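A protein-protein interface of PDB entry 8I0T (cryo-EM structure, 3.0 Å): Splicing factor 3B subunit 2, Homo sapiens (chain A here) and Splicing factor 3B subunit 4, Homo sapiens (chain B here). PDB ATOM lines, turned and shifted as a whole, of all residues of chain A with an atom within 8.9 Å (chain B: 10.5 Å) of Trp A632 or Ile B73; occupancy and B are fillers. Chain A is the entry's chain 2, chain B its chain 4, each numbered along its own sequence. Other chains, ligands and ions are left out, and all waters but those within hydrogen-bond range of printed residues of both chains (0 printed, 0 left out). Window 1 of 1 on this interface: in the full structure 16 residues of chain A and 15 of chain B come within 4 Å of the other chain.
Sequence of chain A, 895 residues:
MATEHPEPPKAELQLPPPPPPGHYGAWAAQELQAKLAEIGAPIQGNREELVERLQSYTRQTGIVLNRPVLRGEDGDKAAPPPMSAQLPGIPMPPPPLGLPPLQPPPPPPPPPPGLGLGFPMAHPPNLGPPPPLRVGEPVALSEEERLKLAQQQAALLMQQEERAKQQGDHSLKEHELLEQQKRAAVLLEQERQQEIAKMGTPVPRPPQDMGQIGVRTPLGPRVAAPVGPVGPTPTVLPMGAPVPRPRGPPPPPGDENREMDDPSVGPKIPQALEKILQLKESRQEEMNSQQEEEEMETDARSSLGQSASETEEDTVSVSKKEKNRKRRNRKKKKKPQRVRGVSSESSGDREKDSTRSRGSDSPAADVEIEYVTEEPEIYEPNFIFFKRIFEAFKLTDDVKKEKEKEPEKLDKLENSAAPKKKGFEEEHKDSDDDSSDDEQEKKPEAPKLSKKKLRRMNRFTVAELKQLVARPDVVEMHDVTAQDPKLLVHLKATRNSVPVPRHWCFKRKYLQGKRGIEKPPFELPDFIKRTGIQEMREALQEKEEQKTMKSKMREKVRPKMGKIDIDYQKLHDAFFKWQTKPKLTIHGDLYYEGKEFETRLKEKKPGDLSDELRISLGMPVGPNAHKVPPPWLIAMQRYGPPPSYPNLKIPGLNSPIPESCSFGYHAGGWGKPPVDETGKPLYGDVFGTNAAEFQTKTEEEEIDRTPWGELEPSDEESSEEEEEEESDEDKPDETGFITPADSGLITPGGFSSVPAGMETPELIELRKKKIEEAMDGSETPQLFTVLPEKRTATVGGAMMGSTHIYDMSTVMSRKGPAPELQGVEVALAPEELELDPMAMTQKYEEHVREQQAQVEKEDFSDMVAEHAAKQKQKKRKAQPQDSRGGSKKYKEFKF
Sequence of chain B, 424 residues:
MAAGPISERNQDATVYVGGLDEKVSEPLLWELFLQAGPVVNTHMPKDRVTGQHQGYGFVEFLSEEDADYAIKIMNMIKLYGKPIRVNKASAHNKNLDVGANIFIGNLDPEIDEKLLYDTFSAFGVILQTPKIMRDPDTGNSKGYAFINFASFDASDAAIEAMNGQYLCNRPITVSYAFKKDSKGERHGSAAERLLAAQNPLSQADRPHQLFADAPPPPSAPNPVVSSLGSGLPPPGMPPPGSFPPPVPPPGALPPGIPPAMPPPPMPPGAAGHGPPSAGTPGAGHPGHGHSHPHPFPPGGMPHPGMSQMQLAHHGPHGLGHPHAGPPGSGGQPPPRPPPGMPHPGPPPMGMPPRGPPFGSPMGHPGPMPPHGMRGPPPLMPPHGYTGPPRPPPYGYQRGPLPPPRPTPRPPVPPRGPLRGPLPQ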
ATOM      1  N   PRO A 606       8.442 -10.892  32.961  1.00  0.00           N
ATOM      2  CA  PRO A 606       8.112 -11.285  31.585  1.00  0.00           C
ATOM      3  C   PRO A 606       7.332 -10.230  30.825  1.00  0.00           C
ATOM      4  O   PRO A 606       7.585 -10.029  29.631  1.00  0.00           O
ATOM      5  CB  PRO A 606       7.288 -12.565  31.778  1.00  0.00           C
ATOM      6  N   LEU A 617       9.940  -8.147  16.442  1.00  0.00           N
ATOM      7  CA  LEU A 617       9.616  -9.525  16.772  1.00  0.00           C
ATOM      8  C   LEU A 617       8.336 -10.002  16.101  1.00  0.00           C
ATOM      9  O   LEU A 617       8.049 -11.203  16.124  1.00  0.00           O
ATOM     10  CB  LEU A 617       9.492  -9.691  18.290  1.00  0.00           C
ATOM     11  N   MET A 619       5.188  -8.511  16.841  1.00  0.00           N
ATOM     12  CA  MET A 619       4.046  -8.265  17.713  1.00  0.00           C
ATOM     13  C   MET A 619       3.655  -6.791  17.687  1.00  0.00           C
ATOM     14  O   MET A 619       4.343  -5.972  17.070  1.00  0.00           O
ATOM     15  CB  MET A 619       4.333  -8.686  19.162  1.00  0.00           C
ATOM     16  N   VAL A 628      -1.941  -8.429  22.566  1.00  0.00           N
ATOM     17  CA  VAL A 628      -0.988  -9.103  21.692  1.00  0.00           C
ATOM     18  C   VAL A 628      -0.187 -10.078  22.551  1.00  0.00           C
ATOM     19  O   VAL A 628       0.691  -9.637  23.312  1.00  0.00           O
ATOM     20  CB  VAL A 628      -0.065  -8.102  20.984  1.00  0.00           C
ATOM     21  N   PRO A 629      -0.461 -11.376  22.489  1.00  0.00           N
ATOM     22  CA  PRO A 629       0.467 -12.343  23.059  1.00  0.00           C
ATOM     23  C   PRO A 629       1.667 -12.504  22.146  1.00  0.00           C
ATOM     24  O   PRO A 629       1.511 -12.796  20.950  1.00  0.00           O
ATOM     25  CB  PRO A 629      -0.366 -13.631  23.134  1.00  0.00           C
ATOM     26  N   PRO A 630       2.878 -12.307  22.661  1.00  0.00           N
ATOM     27  CA  PRO A 630       4.058 -12.291  21.791  1.00  0.00           C
ATOM     28  C   PRO A 630       4.345 -13.674  21.229  1.00  0.00           C
ATOM     29  O   PRO A 630       3.790 -14.676  21.704  1.00  0.00           O
ATOM     30  CB  PRO A 630       5.179 -11.819  22.730  1.00  0.00           C
ATOM     31  N   PRO A 631       5.206 -13.772  20.210  1.00  0.00           N
ATOM     32  CA  PRO A 631       5.471 -15.086  19.597  1.00  0.00           C
ATOM     33  C   PRO A 631       6.124 -16.089  20.538  1.00  0.00           C
ATOM     34  O   PRO A 631       6.256 -17.265  20.167  1.00  0.00           O
ATOM     35  CB  PRO A 631       6.393 -14.745  18.417  1.00  0.00           C
ATOM     36  N   TRP A 632       6.535 -15.668  21.736  1.00  0.00           N
ATOM     37  CA  TRP A 632       7.076 -16.591  22.723  1.00  0.00           C
ATOM     38  C   TRP A 632       6.003 -17.154  23.646  1.00  0.00           C
ATOM     39  O   TRP A 632       6.155 -18.276  24.143  1.00  0.00           O
ATOM     40  CB  TRP A 632       8.162 -15.898  23.551  1.00  0.00           C
ATOM     41  N   LEU A 633       4.903 -16.421  23.850  1.00  0.00           N
ATOM     42  CA  LEU A 633       3.765 -16.994  24.560  1.00  0.00           C
ATOM     43  C   LEU A 633       3.112 -18.112  23.755  1.00  0.00           C
ATOM     44  O   LEU A 633       2.413 -18.956  24.326  1.00  0.00           O
ATOM     45  CB  LEU A 633       2.742 -15.908  24.893  1.00  0.00           C
ATOM     46  N   ILE A 634       3.360 -18.159  22.444  1.00  0.00           N
ATOM     47  CA  ILE A 634       2.828 -19.240  21.616  1.00  0.00           C
ATOM     48  C   ILE A 634       3.432 -20.575  22.038  1.00  0.00           C
ATOM     49  O   ILE A 634       2.718 -21.543  22.323  1.00  0.00           O
ATOM     50  CB  ILE A 634       3.075 -18.952  20.126  1.00  0.00           C
ATOM     51  N   ALA A 635       4.762 -20.647  22.118  1.00  0.00           N
ATOM     52  CA  ALA A 635       5.350 -21.890  22.604  1.00  0.00           C
ATOM     53  C   ALA A 635       5.315 -21.995  24.121  1.00  0.00           C
ATOM     54  O   ALA A 635       5.507 -23.094  24.646  1.00  0.00           O
ATOM     55  CB  ALA A 635       6.778 -22.060  22.109  1.00  0.00           C
ATOM     56  N   MET A 636       5.053 -20.898  24.837  1.00  0.00           N
ATOM     57  CA  MET A 636       4.643 -21.033  26.229  1.00  0.00           C
ATOM     58  C   MET A 636       3.387 -21.890  26.330  1.00  0.00           C
ATOM     59  O   MET A 636       3.332 -22.847  27.108  1.00  0.00           O
ATOM     60  CB  MET A 636       4.406 -19.658  26.848  1.00  0.00           C
ATOM     61  N   GLN A 637       2.378 -21.579  25.519  1.00  0.00           N
ATOM     62  CA  GLN A 637       1.182 -22.412  25.479  1.00  0.00           C
ATOM     63  C   GLN A 637       1.477 -23.792  24.899  1.00  0.00           C
ATOM     64  O   GLN A 637       0.813 -24.774  25.261  1.00  0.00           O
ATOM     65  CB  GLN A 637       0.087 -21.711  24.673  1.00  0.00           C
ATOM     66  N   ARG A 638       2.475 -23.890  24.014  1.00  0.00           N
ATOM     67  CA  ARG A 638       2.736 -25.141  23.304  1.00  0.00           C
ATOM     68  C   ARG A 638       3.459 -26.172  24.173  1.00  0.00           C
ATOM     69  O   ARG A 638       3.031 -27.328  24.249  1.00  0.00           O
ATOM     70  CB  ARG A 638       3.537 -24.858  22.032  1.00  0.00           C
ATOM     71  N   TYR A 639       4.556 -25.783  24.834  1.00  0.00           N
ATOM     72  CA  TYR A 639       5.334 -26.720  25.641  1.00  0.00           C
ATOM     73  C   TYR A 639       5.749 -26.124  26.985  1.00  0.00           C
ATOM     74  O   TYR A 639       6.536 -26.729  27.716  1.00  0.00           O
ATOM     75  CB  TYR A 639       6.563 -27.206  24.871  1.00  0.00           C
ATOM     76  N   GLY A 640       5.225 -24.953  27.340  1.00  0.00           N
ATOM     77  CA  GLY A 640       5.452 -24.378  28.644  1.00  0.00           C
ATOM     78  C   GLY A 640       6.307 -23.125  28.636  1.00  0.00           C
ATOM     79  O   GLY A 640       7.121 -22.899  27.736  1.00  0.00           O
ATOM     80  N   PRO A 641       6.127 -22.280  29.648  1.00  0.00           N
ATOM     81  CA  PRO A 641       7.018 -21.127  29.829  1.00  0.00           C
ATOM     82  C   PRO A 641       8.348 -21.575  30.405  1.00  0.00           C
ATOM     83  O   PRO A 641       8.440 -22.668  30.984  1.00  0.00           O
ATOM     84  CB  PRO A 641       6.250 -20.235  30.816  1.00  0.00           C
ATOM     85  N   PRO A 642       9.397 -20.765  30.267  1.00  0.00           N
ATOM     86  CA  PRO A 642      10.762 -21.251  30.524  1.00  0.00           C
ATOM     87  C   PRO A 642      10.946 -21.684  31.966  1.00  0.00           C
ATOM     88  O   PRO A 642      10.435 -21.039  32.892  1.00  0.00           O
ATOM     89  CB  PRO A 642      11.637 -20.040  30.189  1.00  0.00           C
ATOM     90  N   ILE A 650       2.433 -16.197  31.571  1.00  0.00           N
ATOM     91  CA  ILE A 650       2.370 -15.537  30.270  1.00  0.00           C
ATOM     92  C   ILE A 650       0.943 -15.055  30.027  1.00  0.00           C
ATOM     93  O   ILE A 650      -0.017 -15.772  30.341  1.00  0.00           O
ATOM     94  CB  ILE A 650       2.851 -16.469  29.146  1.00  0.00           C
ATOM     95  N   PRO A 651       0.758 -13.845  29.477  1.00  0.00           N
ATOM     96  CA  PRO A 651      -0.599 -13.299  29.335  1.00  0.00           C
ATOM     97  C   PRO A 651      -1.305 -13.827  28.099  1.00  0.00           C
ATOM     98  O   PRO A 651      -0.869 -13.590  26.970  1.00  0.00           O
ATOM     99  CB  PRO A 651      -0.360 -11.788  29.249  1.00  0.00           C
ATOM    100  N   LEU A 653      -1.523 -17.073  27.769  1.00  0.00           N
ATOM    101  CA  LEU A 653      -0.992 -18.428  27.733  1.00  0.00           C
ATOM    102  C   LEU A 653      -1.045 -19.101  29.093  1.00  0.00           C
ATOM    103  O   LEU A 653      -1.378 -20.290  29.183  1.00  0.00           O
ATOM    104  CB  LEU A 653       0.454 -18.415  27.217  1.00  0.00           C
ATOM    105  N   VAL B  15      22.875 -20.425  23.365  1.00  0.00           N
ATOM    106  CA  VAL B  15      21.872 -20.598  22.325  1.00  0.00           C
ATOM    107  C   VAL B  15      22.318 -19.844  21.081  1.00  0.00           C
ATOM    108  O   VAL B  15      22.757 -18.692  21.165  1.00  0.00           O
ATOM    109  CB  VAL B  15      20.485 -20.102  22.782  1.00  0.00           C
ATOM    110  N   LEU B  28      16.950  -5.011  22.995  1.00  0.00           N
ATOM    111  CA  LEU B  28      15.662  -5.694  23.043  1.00  0.00           C
ATOM    112  C   LEU B  28      15.839  -7.207  22.997  1.00  0.00           C
ATOM    113  O   LEU B  28      14.984  -7.953  23.484  1.00  0.00           O
ATOM    114  CB  LEU B  28      14.770  -5.224  21.896  1.00  0.00           C
ATOM    115  N   LEU B  29      16.940  -7.679  22.408  1.00  0.00           N
ATOM    116  CA  LEU B  29      17.271  -9.097  22.475  1.00  0.00           C
ATOM    117  C   LEU B  29      17.400  -9.560  23.923  1.00  0.00           C
ATOM    118  O   LEU B  29      16.818 -10.575  24.322  1.00  0.00           O
ATOM    119  CB  LEU B  29      18.560  -9.367  21.700  1.00  0.00           C
ATOM    120  N   GLU B  31      16.208  -7.879  26.516  1.00  0.00           N
ATOM    121  CA  GLU B  31      14.923  -7.665  27.171  1.00  0.00           C
ATOM    122  C   GLU B  31      13.965  -8.828  26.924  1.00  0.00           C
ATOM    123  O   GLU B  31      13.208  -9.206  27.824  1.00  0.00           O
ATOM    124  CB  GLU B  31      14.301  -6.350  26.700  1.00  0.00           C
ATOM    125  N   LEU B  32      13.997  -9.425  25.733  1.00  0.00           N
ATOM    126  CA  LEU B  32      13.242 -10.648  25.497  1.00  0.00           C
ATOM    127  C   LEU B  32      13.861 -11.826  26.237  1.00  0.00           C
ATOM    128  O   LEU B  32      13.142 -12.707  26.723  1.00  0.00           O
ATOM    129  CB  LEU B  32      13.159 -10.932  23.998  1.00  0.00           C
ATOM    130  N   PHE B  33      15.192 -11.853  26.340  1.00  0.00           N
ATOM    131  CA  PHE B  33      15.850 -12.869  27.158  1.00  0.00           C
ATOM    132  C   PHE B  33      15.334 -12.842  28.590  1.00  0.00           C
ATOM    133  O   PHE B  33      15.072 -13.897  29.178  1.00  0.00           O
ATOM    134  CB  PHE B  33      17.365 -12.664  27.134  1.00  0.00           C
ATOM    135  N   LEU B  34      15.169 -11.646  29.157  1.00  0.00           N
ATOM    136  CA  LEU B  34      14.603 -11.507  30.494  1.00  0.00           C
ATOM    137  C   LEU B  34      13.115 -11.838  30.513  1.00  0.00           C
ATOM    138  O   LEU B  34      12.652 -12.567  31.397  1.00  0.00           O
ATOM    139  CB  LEU B  34      14.839 -10.093  31.020  1.00  0.00           C
ATOM    140  N   GLN B  35      12.351 -11.324  29.547  1.00  0.00           N
ATOM    141  CA  GLN B  35      10.927 -11.624  29.482  1.00  0.00           C
ATOM    142  C   GLN B  35      10.660 -13.110  29.267  1.00  0.00           C
ATOM    143  O   GLN B  35       9.502 -13.538  29.320  1.00  0.00           O
ATOM    144  CB  GLN B  35      10.273 -10.799  28.371  1.00  0.00           C
ATOM    145  N   ALA B  36      11.701 -13.892  28.992  1.00  0.00           N
ATOM    146  CA  ALA B  36      11.578 -15.341  28.969  1.00  0.00           C
ATOM    147  C   ALA B  36      12.175 -16.010  30.197  1.00  0.00           C
ATOM    148  O   ALA B  36      11.635 -17.018  30.661  1.00  0.00           O
ATOM    149  CB  ALA B  36      12.247 -15.914  27.714  1.00  0.00           C
ATOM    150  N   GLY B  37      13.256 -15.471  30.744  1.00  0.00           N
ATOM    151  CA  GLY B  37      13.935 -16.099  31.849  1.00  0.00           C
ATOM    152  C   GLY B  37      15.235 -15.408  32.207  1.00  0.00           C
ATOM    153  O   GLY B  37      15.349 -14.180  32.188  1.00  0.00           O
ATOM    154  N   GLU B  65      17.299 -25.500  31.173  1.00  0.00           N
ATOM    155  CA  GLU B  65      15.909 -25.651  30.754  1.00  0.00           C
ATOM    156  C   GLU B  65      15.271 -24.300  30.444  1.00  0.00           C
ATOM    157  O   GLU B  65      14.390 -24.213  29.574  1.00  0.00           O
ATOM    158  CB  GLU B  65      15.109 -26.394  31.825  1.00  0.00           C
ATOM    159  N   ASP B  66      15.697 -23.241  31.138  1.00  0.00           N
ATOM    160  CA  ASP B  66      15.244 -21.899  30.792  1.00  0.00           C
ATOM    161  C   ASP B  66      15.577 -21.573  29.349  1.00  0.00           C
ATOM    162  O   ASP B  66      14.711 -21.132  28.586  1.00  0.00           O
ATOM    163  CB  ASP B  66      15.883 -20.867  31.713  1.00  0.00           C
ATOM    164  N   ALA B  67      16.844 -21.758  28.967  1.00  0.00           N
ATOM    165  CA  ALA B  67      17.243 -21.517  27.587  1.00  0.00           C
ATOM    166  C   ALA B  67      16.521 -22.456  26.635  1.00  0.00           C
ATOM    167  O   ALA B  67      16.181 -22.058  25.521  1.00  0.00           O
ATOM    168  CB  ALA B  67      18.757 -21.668  27.437  1.00  0.00           C
ATOM    169  N   ASP B  68      16.235 -23.683  27.072  1.00  0.00           N
ATOM    170  CA  ASP B  68      15.564 -24.646  26.205  1.00  0.00           C
ATOM    171  C   ASP B  68      14.163 -24.172  25.835  1.00  0.00           C
ATOM    172  O   ASP B  68      13.812 -24.082  24.651  1.00  0.00           O
ATOM    173  CB  ASP B  68      15.511 -26.009  26.894  1.00  0.00           C
ATOM    174  N   TYR B  69      13.345 -23.863  26.844  1.00  0.00           N
ATOM    175  CA  TYR B  69      11.987 -23.399  26.573  1.00  0.00           C
ATOM    176  C   TYR B  69      11.961 -21.995  25.976  1.00  0.00           C
ATOM    177  O   TYR B  69      11.119 -21.718  25.110  1.00  0.00           O
ATOM    178  CB  TYR B  69      11.149 -23.449  27.849  1.00  0.00           C
ATOM    179  N   ALA B  70      12.877 -21.117  26.388  1.00  0.00           N
ATOM    180  CA  ALA B  70      13.018 -19.820  25.740  1.00  0.00           C
ATOM    181  C   ALA B  70      13.339 -19.981  24.260  1.00  0.00           C
ATOM    182  O   ALA B  70      12.900 -19.180  23.430  1.00  0.00           O
ATOM    183  CB  ALA B  70      14.102 -19.003  26.447  1.00  0.00           C
ATOM    184  N   ILE B  71      14.100 -21.019  23.911  1.00  0.00           N
ATOM    185  CA  ILE B  71      14.420 -21.272  22.513  1.00  0.00           C
ATOM    186  C   ILE B  71      13.195 -21.789  21.778  1.00  0.00           C
ATOM    187  O   ILE B  71      12.857 -21.313  20.686  1.00  0.00           O
ATOM    188  CB  ILE B  71      15.595 -22.261  22.416  1.00  0.00           C
ATOM    189  N   LYS B  72      12.507 -22.763  22.372  1.00  0.00           N
ATOM    190  CA  LYS B  72      11.283 -23.263  21.764  1.00  0.00           C
ATOM    191  C   LYS B  72      10.293 -22.135  21.526  1.00  0.00           C
ATOM    192  O   LYS B  72       9.489 -22.204  20.590  1.00  0.00           O
ATOM    193  CB  LYS B  72      10.662 -24.347  22.646  1.00  0.00           C
ATOM    194  N   ILE B  73      10.362 -21.081  22.339  1.00  0.00           N
ATOM    195  CA  ILE B  73       9.422 -19.969  22.252  1.00  0.00           C
ATOM    196  C   ILE B  73       9.866 -18.927  21.230  1.00  0.00           C
ATOM    197  O   ILE B  73       9.068 -18.477  20.399  1.00  0.00           O
ATOM    198  CB  ILE B  73       9.222 -19.333  23.641  1.00  0.00           C
ATOM    199  N   MET B  74      11.137 -18.542  21.274  1.00  0.00           N
ATOM    200  CA  MET B  74      11.644 -17.466  20.438  1.00  0.00           C
ATOM    201  C   MET B  74      12.089 -17.949  19.073  1.00  0.00           C
ATOM    202  O   MET B  74      12.583 -17.142  18.279  1.00  0.00           O
ATOM    203  CB  MET B  74      12.807 -16.759  21.134  1.00  0.00           C
ATOM    204  N   ASN B  75      11.946 -19.242  18.792  1.00  0.00           N
ATOM    205  CA  ASN B  75      11.910 -19.688  17.409  1.00  0.00           C
ATOM    206  C   ASN B  75      10.610 -19.207  16.779  1.00  0.00           C
ATOM    207  O   ASN B  75       9.581 -19.118  17.452  1.00  0.00           O
ATOM    208  CB  ASN B  75      12.024 -21.211  17.327  1.00  0.00           C
ATOM    209  N   MET B  76      10.679 -18.842  15.502  1.00  0.00           N
ATOM    210  CA  MET B  76       9.542 -18.345  14.730  1.00  0.00           C
ATOM    211  C   MET B  76       9.092 -16.957  15.169  1.00  0.00           C
ATOM    212  O   MET B  76       8.178 -16.384  14.565  1.00  0.00           O
ATOM    213  CB  MET B  76       8.353 -19.316  14.770  1.00  0.00           C
ATOM    214  N   ILE B  77       9.713 -16.388  16.201  1.00  0.00           N
ATOM    215  CA  ILE B  77       9.490 -14.977  16.502  1.00  0.00           C
ATOM    216  C   ILE B  77      10.023 -14.160  15.333  1.00  0.00           C
ATOM    217  O   ILE B  77      11.132 -14.406  14.839  1.00  0.00           O
ATOM    218  CB  ILE B  77      10.155 -14.576  17.823  1.00  0.00           C
ATOM    219  N   LYS B  78       9.234 -13.194  14.875  1.00  0.00           N
ATOM    220  CA  LYS B  78       9.503 -12.517  13.607  1.00  0.00           C
ATOM    221  C   LYS B  78      10.585 -11.453  13.794  1.00  0.00           C
ATOM    222  O   LYS B  78      10.323 -10.250  13.840  1.00  0.00           O
ATOM    223  CB  LYS B  78       8.218 -11.919  13.051  1.00  0.00           C
ATOM    224  N   LEU B  79      11.829 -11.924  13.881  1.00  0.00           N
ATOM    225  CA  LEU B  79      12.966 -11.016  13.994  1.00  0.00           C
ATOM    226  C   LEU B  79      13.238 -10.344  12.651  1.00  0.00           C
ATOM    227  O   LEU B  79      13.354 -11.012  11.623  1.00  0.00           O
ATOM    228  CB  LEU B  79      14.203 -11.769  14.477  1.00  0.00           C
ATOM    229  N   LYS B  82      11.208 -11.398  10.189  1.00  0.00           N
ATOM    230  CA  LYS B  82      11.503 -12.741   9.717  1.00  0.00           C
ATOM    231  C   LYS B  82      11.621 -13.704  10.894  1.00  0.00           C
ATOM    232  O   LYS B  82      12.137 -13.324  11.949  1.00  0.00           O
ATOM    233  CB  LYS B  82      12.798 -12.745   8.910  1.00  0.00           C
ATOM    234  N   PRO B  83      11.161 -14.944  10.756  1.00  0.00           N
ATOM    235  CA  PRO B  83      11.365 -15.921  11.833  1.00  0.00           C
ATOM    236  C   PRO B  83      12.845 -16.198  12.050  1.00  0.00           C
ATOM    237  O   PRO B  83      13.553 -16.640  11.142  1.00  0.00           O
ATOM    238  CB  PRO B  83      10.618 -17.160  11.327  1.00  0.00           C
ATOM    239  N   ILE B  84      13.315 -15.916  13.259  1.00  0.00           N
ATOM    240  CA  ILE B  84      14.678 -16.246  13.662  1.00  0.00           C
ATOM    241  C   ILE B  84      14.600 -17.244  14.804  1.00  0.00           C
ATOM    242  O   ILE B  84      13.669 -17.198  15.618  1.00  0.00           O
ATOM    243  CB  ILE B  84      15.461 -14.989  14.075  1.00  0.00           C
ATOM    244  N   ARG B  85      15.570 -18.151  14.867  1.00  0.00           N
ATOM    245  CA  ARG B  85      15.474 -19.306  15.748  1.00  0.00           C
ATOM    246  C   ARG B  85      16.556 -19.281  16.821  1.00  0.00           C
ATOM    247  O   ARG B  85      17.713 -18.956  16.547  1.00  0.00           O
ATOM    248  CB  ARG B  85      15.575 -20.594  14.930  1.00  0.00           C
ATOM    249  N   VAL B  86      16.178 -19.640  18.043  1.00  0.00           N
ATOM    250  CA  VAL B  86      17.132 -19.874  19.119  1.00  0.00           C
ATOM    251  C   VAL B  86      17.403 -21.374  19.173  1.00  0.00           C
ATOM    252  O   VAL B  86      16.499 -22.161  19.474  1.00  0.00           O
ATOM    253  CB  VAL B  86      16.612 -19.358  20.470  1.00  0.00           C
ATOM    254  N   ASN B  87      18.642 -21.765  18.896  1.00  0.00           N
ATOM    255  CA  ASN B  87      18.973 -23.173  18.672  1.00  0.00           C
ATOM    256  C   ASN B  87      20.251 -23.499  19.440  1.00  0.00           C
ATOM    257  O   ASN B  87      20.628 -22.779  20.366  1.00  0.00           O
ATOM    258  CB  ASN B  87      19.087 -23.458  17.164  1.00  0.00           C
ATOM    259  N   GLU B 113       0.699 -21.537  14.135  1.00  0.00           N
ATOM    260  CA  GLU B 113       1.924 -21.454  13.344  1.00  0.00           C
ATOM    261  C   GLU B 113       3.159 -21.856  14.145  1.00  0.00           C
ATOM    262  O   GLU B 113       4.049 -22.534  13.619  1.00  0.00           O
ATOM    263  CB  GLU B 113       2.085 -20.044  12.779  1.00  0.00           C
ATOM    264  N   LYS B 114       3.239 -21.468  15.418  1.00  0.00           N
ATOM    265  CA  LYS B 114       4.366 -21.905  16.236  1.00  0.00           C
ATOM    266  C   LYS B 114       4.235 -23.381  16.592  1.00  0.00           C
ATOM    267  O   LYS B 114       5.235 -24.108  16.669  1.00  0.00           O
ATOM    268  CB  LYS B 114       4.476 -21.048  17.495  1.00  0.00           C
ATOM    269  N   LEU B 115       3.003 -23.844  16.814  1.00  0.00           N
ATOM    270  CA  LEU B 115       2.764 -25.276  16.922  1.00  0.00           C
ATOM    271  C   LEU B 115       3.221 -26.007  15.663  1.00  0.00           C
ATOM    272  O   LEU B 115       3.814 -27.087  15.751  1.00  0.00           O
ATOM    273  CB  LEU B 115       1.283 -25.538  17.189  1.00  0.00           C
ATOM    274  N   TYR B 117       5.623 -24.963  13.563  1.00  0.00           N
ATOM    275  CA  TYR B 117       7.082 -24.922  13.527  1.00  0.00           C
ATOM    276  C   TYR B 117       7.685 -25.945  14.480  1.00  0.00           C
ATOM    277  O   TYR B 117       8.711 -26.559  14.171  1.00  0.00           O
ATOM    278  CB  TYR B 117       7.578 -23.519  13.867  1.00  0.00           C
ATOM    279  N   ASP B 118       7.046 -26.157  15.634  1.00  0.00           N
ATOM    280  CA  ASP B 118       7.575 -27.101  16.616  1.00  0.00           C
ATOM    281  C   ASP B 118       7.209 -28.542  16.265  1.00  0.00           C
ATOM    282  O   ASP B 118       7.873 -29.483  16.713  1.00  0.00           O
ATOM    283  CB  ASP B 118       7.073 -26.737  18.014  1.00  0.00           C
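The backbone carbonyl oxygen of Ile B73 lies close to the backbone carbonyl oxygen of Pro A631, at 3.1 Å. The backbone NH of Lys B78 sits at hydrogen-bond distance from the backbone carbonyl oxygen of Leu A617 (2.6 Å).
The backbone carbonyl oxygen (O) of Ile B77 sits at hydrogen-bond distance from the backbone NH (N) of Ile B84, at 3.1 Å. The backbone carbonyl oxygen of Ala A635 is in hydrogen-bond range of the backbone NH of Gly A640 (3.3 Å).
O of Pro A606 touches CB of Gln B35, 3.1 Å away. C of Ile B77 touches O of Leu A617 (3.6 Å). Pro A631 touches Ile B77. Trp A632 touches Ile B73. Lys B114 touches Ile A634. Lys B72 touches Ala A635 (O to CB, 3.1 Å). Ile B73 touches Ala A635. Pro A642 touches Ala B36. CB of Pro A642 touches O of Asp B66, at 3.6 Å. Pro A642 touches Tyr B69 (CA to CB, 3.5 Å).
Of the printed residues of chain B, Pro A606 touches Gln B35 (3.1 Å). No residue of chain B comes within 4 Å of Pro A630. Of chain B, only Ile B73 (3.3 Å) comes within 4 Å of Trp A632. Leu A633 touches none of the printed residues of chain B. Of chain B, only Lys B114 (3.6 Å) comes within 4 Å of Ile A634. Ala A635 touches just these residues of chain B: Lys B72 and Ile B73. Tyr A639 touches none of the printed residues of chain B. Of the printed residues of chain A, Ala B36 touches Pro A642. Printed residues of chain A within 4 Å of Asp B66: Pro A642. Of the printed residues of chain A, Tyr B69 touches Pro A642 (3.5 Å). Lys B72 touches just one residue of chain A: Ala A635 (3.1 Å). Of chain A, only Pro A631, Trp A632 and Ala A635 come within 4 Å of Ile B73. No residue of chain A comes within 4 Å of Met B74. Met B76 touches none of the printed residues of chain A. Printed residues of chain A within 4 Å of Lys B114: Ile A634. The nearest residue of chain A that does not touch Ile B73 is Met A636 (4.6 Å). The nearest printed residue of chain A that does not touch Gln B35 is Trp A632 (6.4 Å).
Of the 21 printed residues of chain A, 7 touch a printed residue of chain B. Hydrophobic or aromatic side chains of chain A that line the printed part of chain B: Pro A606, Pro A631, Trp A632, Ile A634, Ala A635 and Pro A642. Hydrophobic or aromatic side chains of chain B that line the printed part of chain A: Tyr B69, Ile B73 and Ile B77. Among the printed residues, no Asp or Glu carboxylate lies within 4 Å of a Lys or Arg side-chain nitrogen of the other chain.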
